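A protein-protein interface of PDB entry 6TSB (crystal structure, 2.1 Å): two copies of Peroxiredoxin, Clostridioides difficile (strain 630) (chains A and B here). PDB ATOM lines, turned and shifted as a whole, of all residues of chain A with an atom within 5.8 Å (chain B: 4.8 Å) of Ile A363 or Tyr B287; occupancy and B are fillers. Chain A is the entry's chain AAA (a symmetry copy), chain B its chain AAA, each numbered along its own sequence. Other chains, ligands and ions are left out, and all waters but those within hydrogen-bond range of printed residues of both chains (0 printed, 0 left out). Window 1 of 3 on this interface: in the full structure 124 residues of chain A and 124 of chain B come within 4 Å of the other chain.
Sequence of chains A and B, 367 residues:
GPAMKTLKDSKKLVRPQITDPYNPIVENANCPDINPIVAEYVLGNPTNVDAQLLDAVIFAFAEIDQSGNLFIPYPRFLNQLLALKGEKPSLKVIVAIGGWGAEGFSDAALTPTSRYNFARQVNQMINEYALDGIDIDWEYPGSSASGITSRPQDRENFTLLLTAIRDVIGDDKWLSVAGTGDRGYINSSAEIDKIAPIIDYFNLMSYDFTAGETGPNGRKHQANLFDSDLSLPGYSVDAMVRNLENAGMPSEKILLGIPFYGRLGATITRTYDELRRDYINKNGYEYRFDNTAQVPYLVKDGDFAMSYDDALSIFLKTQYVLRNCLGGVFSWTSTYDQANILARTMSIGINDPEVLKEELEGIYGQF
O of Glu A361 sits close to O of Phe B289, at 3.4 Å.
OD2 of Asp B310 lies within hydrogen-bond range of OH of Tyr B287 (2.6 Å).
The backbone NH (N) of Arg B288 lies within hydrogen-bond range of the backbone carbonyl oxygen (O) of Tyr B297, 2.9 Å away.
The side-chain carboxylate (OD2) of Asp B310 lies within hydrogen-bond range of the side-chain hydroxyl (OH) of Tyr B364 (2.8 Å).
Among the printed residues, pairs that only touch across the chains: Ile A280 with Tyr B308 (3.9 Å), Gly A362 with Arg B288 (3.1 Å), Gly A362 with Phe B289 (3.5 Å), Ile A363 with Tyr B287 (3.99 Å), Ile A363 with Arg B288 (3.8 Å), Ile A363 with Phe B289 (3.8 Å), Gly A365 with Phe B289 (3.7 Å) and Gly A365 with Tyr B364 (3.7 Å).
Printed residues of chain B within 4 Å of Gly A362: Arg B288 and Phe B289.
Of the printed residues of chain B, Ile A363 touches Tyr B287 (3.99 Å), Arg B288 (3.8 Å) and Phe B289 (3.8 Å).
Of the printed residues of chain B, Gly A365 touches Phe B289 and Tyr B364.
Glu B286 touches none of the printed residues of chain A.
Of the printed residues of chain A, Tyr B287 touches Ile A363 (3.99 Å).
Of the printed residues of chain A, Arg B288 touches Gly A362 (3.1 Å) and Ile A363 (3.8 Å).
Of the printed residues of chain A, Tyr B308 touches Ile A280.
Asp B310 touches none of the printed residues of chain A.
The nearest printed residue of chain B that does not touch Ile A363 is Tyr B297 (6.0 Å).
The nearest printed residue of chain B that does not touch Gly A365 is Tyr B287 (5.3 Å).
Printed residues of chain B that touch a printed residue of chain A: Tyr B287, Arg B288, Phe B289, Tyr B308 and Tyr B364.
Hydrophobic or aromatic side chains of chain A within 4 Å of the printed part of chain B: Ile A280 and Ile A363.
Along chain A the printed residues that touch a printed residue of chain B span positions 280 to 365.
Position printed for both chains: 364.
Of the 9 pairs that touch across the chains among the printed residues, none has its exchanged pair printed and touching as well.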
ATOM      1  N   ILE A 280      15.744   5.853  25.052  1.00  0.00           N
ATOM      2  CA  ILE A 280      16.972   5.635  24.218  1.00  0.00           C
ATOM      3  C   ILE A 280      16.948   4.346  23.363  1.00  0.00           C
ATOM      4  O   ILE A 280      17.239   4.467  22.131  1.00  0.00           O
ATOM      5  CB  ILE A 280      18.258   5.827  25.055  1.00  0.00           C
ATOM      6  CG1 ILE A 280      18.600   4.654  25.982  1.00  0.00           C
ATOM      7  CG2 ILE A 280      18.185   7.143  25.828  1.00  0.00           C
ATOM      8  CD1 ILE A 280      19.919   4.849  26.733  1.00  0.00           C
ATOM      9  N   GLU A 359      26.004  18.765   9.926  1.00  0.00           N
ATOM     10  CA  GLU A 359      24.834  17.998  10.449  1.00  0.00           C
ATOM     11  C   GLU A 359      25.290  16.863  11.384  1.00  0.00           C
ATOM     12  O   GLU A 359      24.727  16.731  12.489  1.00  0.00           O
ATOM     13  CB  GLU A 359      24.044  17.420   9.282  1.00  0.00           C
ATOM     14  CG  GLU A 359      22.543  17.509   9.456  1.00  0.00           C
ATOM     15  CD  GLU A 359      21.815  17.620   8.127  1.00  0.00           C
ATOM     16  OE1 GLU A 359      22.029  18.624   7.412  1.00  0.00           O
ATOM     17  OE2 GLU A 359      21.070  16.690   7.800  1.00  0.00           O
ATOM     18  N   LEU A 360      26.272  16.062  10.963  1.00  0.00           N
ATOM     19  CA  LEU A 360      26.665  14.803  11.653  1.00  0.00           C
ATOM     20  C   LEU A 360      27.624  15.099  12.822  1.00  0.00           C
ATOM     21  O   LEU A 360      27.787  14.191  13.689  1.00  0.00           O
ATOM     22  CB  LEU A 360      27.314  13.834  10.651  1.00  0.00           C
ATOM     23  CG  LEU A 360      26.496  13.399   9.422  1.00  0.00           C
ATOM     24  CD1 LEU A 360      27.324  12.490   8.528  1.00  0.00           C
ATOM     25  CD2 LEU A 360      25.202  12.690   9.784  1.00  0.00           C
ATOM     26  N   GLU A 361      28.263  16.281  12.839  1.00  0.00           N
ATOM     27  CA  GLU A 361      29.099  16.776  13.979  1.00  0.00           C
ATOM     28  C   GLU A 361      28.192  16.939  15.204  1.00  0.00           C
ATOM     29  O   GLU A 361      28.698  16.780  16.328  1.00  0.00           O
ATOM     30  CB  GLU A 361      29.819  18.102  13.675  1.00  0.00           C
ATOM     31  CG  GLU A 361      31.166  17.993  12.945  1.00  0.00           C
ATOM     32  CD  GLU A 361      32.317  17.275  13.651  1.00  0.00           C
ATOM     33  OE1 GLU A 361      32.189  16.953  14.855  1.00  0.00           O
ATOM     34  OE2 GLU A 361      33.355  17.048  12.992  1.00  0.00           O
ATOM     35  N   GLY A 362      26.901  17.218  14.972  1.00  0.00           N
ATOM     36  CA  GLY A 362      25.864  17.407  16.002  1.00  0.00           C
ATOM     37  C   GLY A 362      25.018  16.168  16.231  1.00  0.00           C
ATOM     38  O   GLY A 362      23.855  16.334  16.618  1.00  0.00           O
ATOM     39  N   ILE A 363      25.558  14.969  16.008  1.00  0.00           N
ATOM     40  CA  ILE A 363      24.816  13.672  16.140  1.00  0.00           C
ATOM     41  C   ILE A 363      25.762  12.556  16.628  1.00  0.00           C
ATOM     42  O   ILE A 363      25.367  11.768  17.525  1.00  0.00           O
ATOM     43  CB  ILE A 363      24.148  13.268  14.805  1.00  0.00           C
ATOM     44  CG1 ILE A 363      23.134  14.308  14.309  1.00  0.00           C
ATOM     45  CG2 ILE A 363      23.524  11.884  14.942  1.00  0.00           C
ATOM     46  CD1 ILE A 363      22.609  14.060  12.910  1.00  0.00           C
ATOM     47  N   TYR A 364      26.937  12.434  16.012  1.00  0.00           N
ATOM     48  CA  TYR A 364      27.867  11.303  16.239  1.00  0.00           C
ATOM     49  C   TYR A 364      28.955  11.712  17.228  1.00  0.00           C
ATOM     50  O   TYR A 364      29.748  12.652  16.946  1.00  0.00           O
ATOM     51  CB  TYR A 364      28.413  10.807  14.905  1.00  0.00           C
ATOM     52  CG  TYR A 364      27.332  10.137  14.105  1.00  0.00           C
ATOM     53  CD1 TYR A 364      26.524  10.857  13.231  1.00  0.00           C
ATOM     54  CD2 TYR A 364      27.057   8.787  14.288  1.00  0.00           C
ATOM     55  CE1 TYR A 364      25.513  10.231  12.509  1.00  0.00           C
ATOM     56  CE2 TYR A 364      26.045   8.149  13.580  1.00  0.00           C
ATOM     57  CZ  TYR A 364      25.272   8.872  12.682  1.00  0.00           C
ATOM     58  OH  TYR A 364      24.280   8.240  11.981  1.00  0.00           O
ATOM     59  N   GLY A 365      28.968  10.989  18.351  1.00  0.00           N
ATOM     60  CA  GLY A 365      30.000  11.044  19.397  1.00  0.00           C
ATOM     61  C   GLY A 365      31.360  10.645  18.852  1.00  0.00           C
ATOM     62  O   GLY A 365      31.515   9.463  18.419  1.00  0.00           O
ATOM     63  N   TYR B 285      12.194  10.162  20.436  1.00  0.00           N
ATOM     64  CA  TYR B 285      13.378  10.829  21.045  1.00  0.00           C
ATOM     65  C   TYR B 285      14.617  10.463  20.229  1.00  0.00           C
ATOM     66  O   TYR B 285      14.921   9.260  20.026  1.00  0.00           O
ATOM     67  CB  TYR B 285      13.557  10.450  22.518  1.00  0.00           C
ATOM     68  CG  TYR B 285      12.664  11.199  23.472  1.00  0.00           C
ATOM     69  CD1 TYR B 285      12.916  12.526  23.784  1.00  0.00           C
ATOM     70  CD2 TYR B 285      11.565  10.592  24.064  1.00  0.00           C
ATOM     71  CE1 TYR B 285      12.107  13.233  24.658  1.00  0.00           C
ATOM     72  CE2 TYR B 285      10.748  11.284  24.947  1.00  0.00           C
ATOM     73  CZ  TYR B 285      11.016  12.612  25.239  1.00  0.00           C
ATOM     74  OH  TYR B 285      10.225  13.313  26.097  1.00  0.00           O
ATOM     75  N   GLU B 286      15.316  11.491  19.755  1.00  0.00           N
ATOM     76  CA  GLU B 286      16.500  11.326  18.881  1.00  0.00           C
ATOM     77  C   GLU B 286      17.757  11.634  19.704  1.00  0.00           C
ATOM     78  O   GLU B 286      17.765  12.653  20.430  1.00  0.00           O
ATOM     79  CB  GLU B 286      16.324  12.204  17.640  1.00  0.00           C
ATOM     80  CG  GLU B 286      16.889  11.579  16.375  1.00  0.00           C
ATOM     81  CD  GLU B 286      16.022  11.701  15.135  1.00  0.00           C
ATOM     82  OE1 GLU B 286      14.848  12.120  15.251  1.00  0.00           O
ATOM     83  OE2 GLU B 286      16.527  11.357  14.056  1.00  0.00           O
ATOM     84  N   TYR B 287      18.759  10.760  19.607  1.00  0.00           N
ATOM     85  CA  TYR B 287      20.082  10.873  20.270  1.00  0.00           C
ATOM     86  C   TYR B 287      20.953  11.862  19.482  1.00  0.00           C
ATOM     87  O   TYR B 287      21.107  11.683  18.253  1.00  0.00           O
ATOM     88  CB  TYR B 287      20.718   9.487  20.363  1.00  0.00           C
ATOM     89  CG  TYR B 287      22.076   9.459  21.004  1.00  0.00           C
ATOM     90  CD1 TYR B 287      23.210   9.798  20.280  1.00  0.00           C
ATOM     91  CD2 TYR B 287      22.237   9.086  22.332  1.00  0.00           C
ATOM     92  CE1 TYR B 287      24.472   9.744  20.851  1.00  0.00           C
ATOM     93  CE2 TYR B 287      23.492   9.048  22.926  1.00  0.00           C
ATOM     94  CZ  TYR B 287      24.616   9.377  22.182  1.00  0.00           C
ATOM     95  OH  TYR B 287      25.864   9.340  22.741  1.00  0.00           O
ATOM     96  N   ARG B 288      21.479  12.887  20.168  1.00  0.00           N
ATOM     97  CA  ARG B 288      22.414  13.913  19.622  1.00  0.00           C
ATOM     98  C   ARG B 288      23.656  14.003  20.521  1.00  0.00           C
ATOM     99  O   ARG B 288      23.593  13.567  21.702  1.00  0.00           O
ATOM    100  CB  ARG B 288      21.728  15.282  19.534  1.00  0.00           C
ATOM    101  CG  ARG B 288      20.520  15.339  18.611  1.00  0.00           C
ATOM    102  CD  ARG B 288      20.925  15.453  17.157  1.00  0.00           C
ATOM    103  NE  ARG B 288      19.813  15.141  16.266  1.00  0.00           N
ATOM    104  CZ  ARG B 288      18.984  16.028  15.720  1.00  0.00           C
ATOM    105  NH1 ARG B 288      19.118  17.322  15.965  1.00  0.00           N
ATOM    106  NH2 ARG B 288      18.009  15.607  14.932  1.00  0.00           N
ATOM    107  N   PHE B 289      24.752  14.548  19.993  1.00  0.00           N
ATOM    108  CA  PHE B 289      26.051  14.700  20.709  1.00  0.00           C
ATOM    109  C   PHE B 289      26.680  16.075  20.404  1.00  0.00           C
ATOM    110  O   PHE B 289      26.840  16.498  19.216  1.00  0.00           O
ATOM    111  CB  PHE B 289      27.005  13.527  20.421  1.00  0.00           C
ATOM    112  CG  PHE B 289      28.003  13.283  21.521  1.00  0.00           C
ATOM    113  CD1 PHE B 289      29.146  14.057  21.619  1.00  0.00           C
ATOM    114  CD2 PHE B 289      27.763  12.329  22.495  1.00  0.00           C
ATOM    115  CE1 PHE B 289      30.046  13.859  22.651  1.00  0.00           C
ATOM    116  CE2 PHE B 289      28.657  12.131  23.536  1.00  0.00           C
ATOM    117  CZ  PHE B 289      29.796  12.897  23.613  1.00  0.00           C
ATOM    118  N   PRO B 296      26.363  13.809  25.795  1.00  0.00           N
ATOM    119  CA  PRO B 296      25.174  13.462  25.007  1.00  0.00           C
ATOM    120  C   PRO B 296      23.945  14.294  25.382  1.00  0.00           C
ATOM    121  O   PRO B 296      23.938  14.886  26.438  1.00  0.00           O
ATOM    122  CB  PRO B 296      24.901  12.000  25.363  1.00  0.00           C
ATOM    123  CG  PRO B 296      25.457  11.878  26.776  1.00  0.00           C
ATOM    124  CD  PRO B 296      26.678  12.776  26.802  1.00  0.00           C
ATOM    125  N   TYR B 297      22.953  14.318  24.501  1.00  0.00           N
ATOM    126  CA  TYR B 297      21.643  14.957  24.751  1.00  0.00           C
ATOM    127  C   TYR B 297      20.603  14.333  23.819  1.00  0.00           C
ATOM    128  O   TYR B 297      20.988  13.559  22.929  1.00  0.00           O
ATOM    129  CB  TYR B 297      21.766  16.477  24.614  1.00  0.00           C
ATOM    130  CG  TYR B 297      21.990  17.054  23.234  1.00  0.00           C
ATOM    131  CD1 TYR B 297      23.206  16.941  22.569  1.00  0.00           C
ATOM    132  CD2 TYR B 297      20.990  17.801  22.621  1.00  0.00           C
ATOM    133  CE1 TYR B 297      23.403  17.522  21.318  1.00  0.00           C
ATOM    134  CE2 TYR B 297      21.168  18.384  21.375  1.00  0.00           C
ATOM    135  CZ  TYR B 297      22.380  18.251  20.717  1.00  0.00           C
ATOM    136  OH  TYR B 297      22.522  18.847  19.486  1.00  0.00           O
ATOM    137  N   LEU B 298      19.331  14.662  24.039  1.00  0.00           N
ATOM    138  CA  LEU B 298      18.184  14.178  23.234  1.00  0.00           C
ATOM    139  C   LEU B 298      17.384  15.371  22.693  1.00  0.00           C
ATOM    140  O   LEU B 298      17.206  16.370  23.443  1.00  0.00           O
ATOM    141  CB  LEU B 298      17.285  13.291  24.099  1.00  0.00           C
ATOM    142  CG  LEU B 298      17.973  12.136  24.821  1.00  0.00           C
ATOM    143  CD1 LEU B 298      16.943  11.141  25.337  1.00  0.00           C
ATOM    144  CD2 LEU B 298      18.987  11.440  23.933  1.00  0.00           C
ATOM    145  N   TYR B 308      22.158  14.328  29.876  1.00  0.00           N
ATOM    146  CA  TYR B 308      22.600  13.234  30.772  1.00  0.00           C
ATOM    147  C   TYR B 308      24.048  12.904  30.424  1.00  0.00           C
ATOM    148  O   TYR B 308      24.627  13.653  29.625  1.00  0.00           O
ATOM    149  CB  TYR B 308      21.639  12.045  30.678  1.00  0.00           C
ATOM    150  CG  TYR B 308      21.588  11.319  29.357  1.00  0.00           C
ATOM    151  CD1 TYR B 308      20.984  11.892  28.248  1.00  0.00           C
ATOM    152  CD2 TYR B 308      22.103  10.038  29.223  1.00  0.00           C
ATOM    153  CE1 TYR B 308      20.933  11.233  27.025  1.00  0.00           C
ATOM    154  CE2 TYR B 308      22.041   9.355  28.017  1.00  0.00           C
ATOM    155  CZ  TYR B 308      21.456   9.956  26.911  1.00  0.00           C
ATOM    156  OH  TYR B 308      21.402   9.308  25.712  1.00  0.00           O
ATOM    157  N   ASP B 310      26.322   9.333  29.269  1.00  0.00           N
ATOM    158  CA  ASP B 310      26.296   7.925  28.779  1.00  0.00           C
ATOM    159  C   ASP B 310      27.725   7.401  28.874  1.00  0.00           C
ATOM    160  O   ASP B 310      28.530   8.037  29.588  1.00  0.00           O
ATOM    161  CB  ASP B 310      25.691   7.829  27.377  1.00  0.00           C
ATOM    162  CG  ASP B 310      26.541   8.463  26.288  1.00  0.00           C
ATOM    163  OD1 ASP B 310      27.587   9.090  26.624  1.00  0.00           O
ATOM    164  OD2 ASP B 310      26.148   8.330  25.104  1.00  0.00           O
ATOM    165  N   TYR B 364      30.364   3.650  18.921  1.00  0.00           N
ATOM    166  CA  TYR B 364      30.341   5.067  18.491  1.00  0.00           C
ATOM    167  C   TYR B 364      30.986   5.206  17.115  1.00  0.00           C
ATOM    168  O   TYR B 364      32.198   4.900  16.949  1.00  0.00           O
ATOM    169  CB  TYR B 364      30.991   5.941  19.558  1.00  0.00           C
ATOM    170  CG  TYR B 364      30.135   5.999  20.790  1.00  0.00           C
ATOM    171  CD1 TYR B 364      30.274   5.067  21.815  1.00  0.00           C
ATOM    172  CD2 TYR B 364      29.118   6.941  20.897  1.00  0.00           C
ATOM    173  CE1 TYR B 364      29.463   5.118  22.944  1.00  0.00           C
ATOM    174  CE2 TYR B 364      28.295   6.999  22.015  1.00  0.00           C
ATOM    175  CZ  TYR B 364      28.471   6.087  23.047  1.00  0.00           C
ATOM    176  OH  TYR B 364      27.662   6.150  24.150  1.00  0.00           O
